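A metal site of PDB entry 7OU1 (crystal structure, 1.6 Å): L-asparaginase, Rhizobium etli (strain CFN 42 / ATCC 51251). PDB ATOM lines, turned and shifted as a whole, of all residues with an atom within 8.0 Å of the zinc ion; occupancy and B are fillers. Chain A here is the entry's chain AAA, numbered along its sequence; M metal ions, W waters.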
ATOM      1  N   ARG A  53     -15.910   6.145   7.864  1.00  0.00           N
ATOM      2  CA  ARG A  53     -14.742   5.685   8.663  1.00  0.00           C
ATOM      3  C   ARG A  53     -13.817   4.857   7.754  1.00  0.00           C
ATOM      4  O   ARG A  53     -13.521   5.290   6.589  1.00  0.00           O
ATOM      5  CB  ARG A  53     -15.243   4.927   9.911  1.00  0.00           C
ATOM      6  CG  ARG A  53     -16.165   5.728  10.809  1.00  0.00           C
ATOM      7  CD  ARG A  53     -15.491   6.876  11.554  1.00  0.00           C
ATOM      8  NE  ARG A  53     -14.440   6.399  12.447  1.00  0.00           N
ATOM      9  CZ  ARG A  53     -14.653   5.817  13.635  1.00  0.00           C
ATOM     10  NH1 ARG A  53     -15.892   5.609  14.042  1.00  0.00           N
ATOM     11  NH2 ARG A  53     -13.630   5.383  14.362  1.00  0.00           N
ATOM     12  N   SER A  54     -13.389   3.670   8.193  1.00  0.00           N
ATOM     13  CA  SER A  54     -12.485   2.812   7.414  1.00  0.00           C
ATOM     14  C   SER A  54     -13.111   2.308   6.117  1.00  0.00           C
ATOM     15  O   SER A  54     -12.367   1.888   5.235  1.00  0.00           O
ATOM     16  CB  SER A  54     -11.954   1.664   8.241  1.00  0.00           C
ATOM     17  OG  SER A  54     -12.999   1.105   9.072  1.00  0.00           O
ATOM     18  N   LYS A  57     -11.671   3.769   2.914  1.00  0.00           N
ATOM     19  CA  LYS A  57     -10.231   3.499   2.578  1.00  0.00           C
ATOM     20  C   LYS A  57      -9.999   3.301   1.079  1.00  0.00           C
ATOM     21  O   LYS A  57      -9.005   3.837   0.566  1.00  0.00           O
ATOM     22  CB  LYS A  57      -9.681   2.413   3.483  1.00  0.00           C
ATOM     23  CG  LYS A  57      -9.251   2.942   4.853  1.00  0.00           C
ATOM     24  CD  LYS A  57      -8.868   1.904   5.871  1.00  0.00           C
ATOM     25  CE  LYS A  57      -8.394   2.533   7.186  1.00  0.00           C
ATOM     26  NZ  LYS A  57      -8.216   1.491   8.210  1.00  0.00           N
ATOM     27  N   GLN A  60      -9.677   6.711  -0.494  1.00  0.00           N
ATOM     28  CA  GLN A  60      -8.401   7.320  -0.059  1.00  0.00           C
ATOM     29  C   GLN A  60      -7.245   6.688  -0.872  1.00  0.00           C
ATOM     30  O   GLN A  60      -6.353   7.450  -1.333  1.00  0.00           O
ATOM     31  CB  GLN A  60      -8.275   7.198   1.454  1.00  0.00           C
ATOM     32  CG  GLN A  60      -9.278   8.081   2.161  1.00  0.00           C
ATOM     33  CD  GLN A  60      -9.420   7.701   3.619  1.00  0.00           C
ATOM     34  OE1 GLN A  60      -9.780   6.561   3.953  1.00  0.00           O
ATOM     35  NE2 GLN A  60      -9.095   8.650   4.477  1.00  0.00           N
ATOM     36  N   ALA A  85      -6.786  -1.331   4.056  1.00  0.00           N
ATOM     37  CA  ALA A  85      -6.983  -2.247   5.197  1.00  0.00           C
ATOM     38  C   ALA A  85      -7.367  -1.535   6.488  1.00  0.00           C
ATOM     39  O   ALA A  85      -6.883  -0.416   6.780  1.00  0.00           O
ATOM     40  CB  ALA A  85      -5.723  -3.015   5.493  1.00  0.00           C
ATOM     41  N   SER A  86      -8.124  -2.276   7.295  1.00  0.00           N
ATOM     42  CA  SER A  86      -8.151  -2.112   8.783  1.00  0.00           C
ATOM     43  C   SER A  86      -7.517  -3.384   9.341  1.00  0.00           C
ATOM     44  O   SER A  86      -8.247  -4.314   9.737  1.00  0.00           O
ATOM     45  CB  SER A  86      -9.559  -1.896   9.323  1.00  0.00           C
ATOM     46  OG  SER A  86     -10.121  -0.743   8.718  1.00  0.00           O
ATOM     47  N   CYS A 113      -0.012   8.510  12.570  1.00  0.00           N
ATOM     48  CA  CYS A 113      -0.983   7.628  13.262  1.00  0.00           C
ATOM     49  C   CYS A 113      -0.344   7.052  14.523  1.00  0.00           C
ATOM     50  O   CYS A 113       0.867   7.054  14.624  1.00  0.00           O
ATOM     51  CB  CYS A 113      -1.471   6.538  12.331  1.00  0.00           C
ATOM     52  SG  CYS A 113      -0.142   5.556  11.586  1.00  0.00           S
ATOM     53  N   SER A 139      -0.481   0.563  13.675  1.00  0.00           N
ATOM     54  CA  SER A 139      -1.857   1.084  13.481  1.00  0.00           C
ATOM     55  C   SER A 139      -2.584   0.254  12.419  1.00  0.00           C
ATOM     56  O   SER A 139      -1.990  -0.012  11.325  1.00  0.00           O
ATOM     57  CB  SER A 139      -1.820   2.520  13.039  1.00  0.00           C
ATOM     58  OG  SER A 139      -3.095   2.942  12.543  1.00  0.00           O
ATOM     59  N   ASN A 140      -3.867  -0.078  12.627  1.00  0.00           N
ATOM     60  CA  ASN A 140      -4.716  -0.744  11.606  1.00  0.00           C
ATOM     61  C   ASN A 140      -4.769   0.102  10.303  1.00  0.00           C
ATOM     62  O   ASN A 140      -5.035  -0.492   9.233  1.00  0.00           O
ATOM     63  CB  ASN A 140      -6.117  -1.032  12.169  1.00  0.00           C
ATOM     64  CG  ASN A 140      -7.039   0.166  12.069  1.00  0.00           C
ATOM     65  OD1 ASN A 140      -7.777   0.313  11.086  1.00  0.00           O
ATOM     66  ND2 ASN A 140      -6.897   1.091  13.011  1.00  0.00           N
ATOM     67  N   CYS A 141      -4.500   1.406  10.378  1.00  0.00           N
ATOM     68  CA  CYS A 141      -4.504   2.384   9.238  1.00  0.00           C
ATOM     69  C   CYS A 141      -3.102   2.594   8.686  1.00  0.00           C
ATOM     70  O   CYS A 141      -2.908   3.515   7.883  1.00  0.00           O
ATOM     71  CB  CYS A 141      -5.066   3.732   9.718  1.00  0.00           C
ATOM     72  SG  CYS A 141      -6.785   3.533  10.259  1.00  0.00           S
ATOM     73  N   SER A 142      -2.091   1.848   9.144  1.00  0.00           N
ATOM     74  CA  SER A 142      -0.682   2.141   8.790  1.00  0.00           C
ATOM     75  C   SER A 142      -0.483   2.159   7.261  1.00  0.00           C
ATOM     76  O   SER A 142       0.288   3.033   6.786  1.00  0.00           O
ATOM     77  CB  SER A 142       0.271   1.205   9.469  1.00  0.00           C
ATOM     78  OG  SER A 142       0.067  -0.122   9.021  1.00  0.00           O
ATOM     79  N   LYS A 144      -2.676   3.022   4.802  1.00  0.00           N
ATOM     80  CA  LYS A 144      -3.245   4.299   4.321  1.00  0.00           C
ATOM     81  C   LYS A 144      -2.266   5.456   4.648  1.00  0.00           C
ATOM     82  O   LYS A 144      -2.021   6.313   3.760  1.00  0.00           O
ATOM     83  CB  LYS A 144      -4.604   4.537   5.004  1.00  0.00           C
ATOM     84  CG  LYS A 144      -5.196   5.909   4.787  1.00  0.00           C
ATOM     85  CD  LYS A 144      -6.544   6.047   5.393  1.00  0.00           C
ATOM     86  CE  LYS A 144      -6.549   5.746   6.867  1.00  0.00           C
ATOM     87  NZ  LYS A 144      -7.811   6.158   7.519  1.00  0.00           N
ATOM     88  N   HIS A 145      -1.731   5.494   5.867  1.00  0.00           N
ATOM     89  CA  HIS A 145      -0.764   6.561   6.295  1.00  0.00           C
ATOM     90  C   HIS A 145       0.518   6.520   5.461  1.00  0.00           C
ATOM     91  O   HIS A 145       0.990   7.583   5.016  1.00  0.00           O
ATOM     92  CB  HIS A 145      -0.476   6.456   7.779  1.00  0.00           C
ATOM     93  CG  HIS A 145      -1.535   7.114   8.566  1.00  0.00           C
ATOM     94  ND1 HIS A 145      -1.338   8.376   9.128  1.00  0.00           N
ATOM     95  CD2 HIS A 145      -2.805   6.725   8.866  1.00  0.00           C
ATOM     96  CE1 HIS A 145      -2.484   8.751   9.731  1.00  0.00           C
ATOM     97  NE2 HIS A 145      -3.380   7.734   9.603  1.00  0.00           N
ATOM     98  N   MET A 148      -0.362   8.023   2.102  1.00  0.00           N
ATOM     99  CA  MET A 148      -0.509   9.500   2.202  1.00  0.00           C
ATOM    100  C   MET A 148       0.861  10.181   2.317  1.00  0.00           C
ATOM    101  O   MET A 148       1.081  11.216   1.659  1.00  0.00           O
ATOM    102  CB  MET A 148      -1.376   9.869   3.387  1.00  0.00           C
ATOM    103  CG  MET A 148      -2.723  10.280   2.892  1.00  0.00           C
ATOM    104  SD  MET A 148      -3.941   9.789   4.002  1.00  0.00           S
ATOM    105  CE  MET A 148      -5.126   9.156   2.793  1.00  0.00           C
ATOM    106  N   THR A 192     -12.368  13.963  12.424  1.00  0.00           N
ATOM    107  CA  THR A 192     -11.002  13.376  12.577  1.00  0.00           C
ATOM    108  C   THR A 192     -11.162  11.940  13.050  1.00  0.00           C
ATOM    109  O   THR A 192     -11.972  11.696  13.994  1.00  0.00           O
ATOM    110  CB  THR A 192     -10.216  14.277  13.512  1.00  0.00           C
ATOM    111  OG1 THR A 192     -10.101  15.567  12.914  1.00  0.00           O
ATOM    112  CG2 THR A 192      -8.828  13.722  13.799  1.00  0.00           C
ATOM    113  N   ASP A 193     -10.429  11.006  12.423  1.00  0.00           N
ATOM    114  CA  ASP A 193     -10.524   9.570  12.776  1.00  0.00           C
ATOM    115  C   ASP A 193      -9.596   9.208  13.950  1.00  0.00           C
ATOM    116  O   ASP A 193      -8.845  10.089  14.446  1.00  0.00           O
ATOM    117  CB  ASP A 193     -10.323   8.683  11.565  1.00  0.00           C
ATOM    118  CG  ASP A 193     -11.269   7.476  11.638  1.00  0.00           C
ATOM    119  OD1 ASP A 193     -11.580   7.031  12.706  1.00  0.00           O
ATOM    120  OD2 ASP A 193     -11.637   6.983  10.583  1.00  0.00           O
ATOM    121  N   GLY A 194      -9.679   7.961  14.370  1.00  0.00           N
ATOM    122  CA  GLY A 194      -8.816   7.373  15.427  1.00  0.00           C
ATOM    123  C   GLY A 194      -7.338   7.459  15.072  1.00  0.00           C
ATOM    124  O   GLY A 194      -6.494   7.640  15.973  1.00  0.00           O
ATOM    125  N   CYS A 195      -7.041   7.374  13.769  1.00  0.00           N
ATOM    126  CA  CYS A 195      -5.637   7.408  13.246  1.00  0.00           C
ATOM    127  C   CYS A 195      -5.192   8.862  13.008  1.00  0.00           C
ATOM    128  O   CYS A 195      -4.061   9.056  12.575  1.00  0.00           O
ATOM    129  CB  CYS A 195      -5.596   6.602  11.938  1.00  0.00           C
ATOM    130  SG  CYS A 195      -6.507   7.400  10.599  1.00  0.00           S
ATOM    131  N   ASN A 196      -6.068   9.853  13.233  1.00  0.00           N
ATOM    132  CA  ASN A 196      -5.752  11.306  13.234  1.00  0.00           C
ATOM    133  C   ASN A 196      -5.709  11.889  11.793  1.00  0.00           C
ATOM    134  O   ASN A 196      -5.213  13.006  11.627  1.00  0.00           O
ATOM    135  CB  ASN A 196      -4.431  11.622  13.940  1.00  0.00           C
ATOM    136  CG  ASN A 196      -4.459  13.001  14.564  1.00  0.00           C
ATOM    137  OD1 ASN A 196      -5.490  13.417  15.106  1.00  0.00           O
ATOM    138  ND2 ASN A 196      -3.338  13.719  14.529  1.00  0.00           N
ATOM    139  N   LEU A 197      -6.345  11.242  10.828  1.00  0.00           N
ATOM    140  CA  LEU A 197      -6.634  11.824   9.500  1.00  0.00           C
ATOM    141  C   LEU A 197      -8.057  12.395   9.463  1.00  0.00           C
ATOM    142  O   LEU A 197      -8.945  11.906  10.174  1.00  0.00           O
ATOM    143  CB  LEU A 197      -6.554  10.700   8.451  1.00  0.00           C
ATOM    144  CG  LEU A 197      -5.147  10.347   8.022  1.00  0.00           C
ATOM    145  CD1 LEU A 197      -5.154   9.088   7.177  1.00  0.00           C
ATOM    146  CD2 LEU A 197      -4.511  11.493   7.288  1.00  0.00           C
ATOM    147  N   PRO A 198      -8.330  13.307   8.540  1.00  0.00           N
ATOM    148  CA  PRO A 198      -9.705  13.704   8.211  1.00  0.00           C
ATOM    149  C   PRO A 198     -10.462  12.461   7.731  1.00  0.00           C
ATOM    150  O   PRO A 198      -9.898  11.626   7.019  1.00  0.00           O
ATOM    151  CB  PRO A 198      -9.552  14.726   7.083  1.00  0.00           C
ATOM    152  CG  PRO A 198      -8.135  15.147   7.106  1.00  0.00           C
ATOM    153  CD  PRO A 198      -7.363  13.971   7.629  1.00  0.00           C
ATOM    154  N   THR A 199     -11.739  12.364   8.140  1.00  0.00           N
ATOM    155  CA  THR A 199     -12.620  11.228   7.811  1.00  0.00           C
ATOM    156  C   THR A 199     -13.980  11.760   7.385  1.00  0.00           C
ATOM    157  O   THR A 199     -14.499  12.679   7.994  1.00  0.00           O
ATOM    158  CB  THR A 199     -12.645  10.226   8.977  1.00  0.00           C
ATOM    159  OG1 THR A 199     -13.186   9.021   8.435  1.00  0.00           O
ATOM    160  CG2 THR A 199     -13.401  10.753  10.174  1.00  0.00           C
HETATM  161 ZN    ZN M   1      -7.653   5.657   9.701  1.00  0.00          ZN
HETATM  162  O   HOH W   1      -9.985   4.877   9.704  1.00  0.00           O
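The backbone NH (N) of Cys 141 is in hydrogen-bond range of the side-chain hydroxyl (OG) of Ser 139 (3.0 Å). The backbone carbonyl oxygen (O) of Cys 195 sits close to a ring nitrogen (NE2) of His 145, 3.3 Å away. SG of Cys 141 lies close to NZ of Lys 57, 3.2 Å away. OD1 of Asn 140 sits close to SG of Cys 141 (3.5 Å).
The zinc ion is bound by NZ of Lys 144 (2.2 Å), SG of Cys 195 (2.3 Å), SG of Cys 141 (2.4 Å) and water W1 (2.5 Å).
Three residues have an atom within 4 Å of the zinc ion: Cys 141, Lys 144 and Cys 195.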
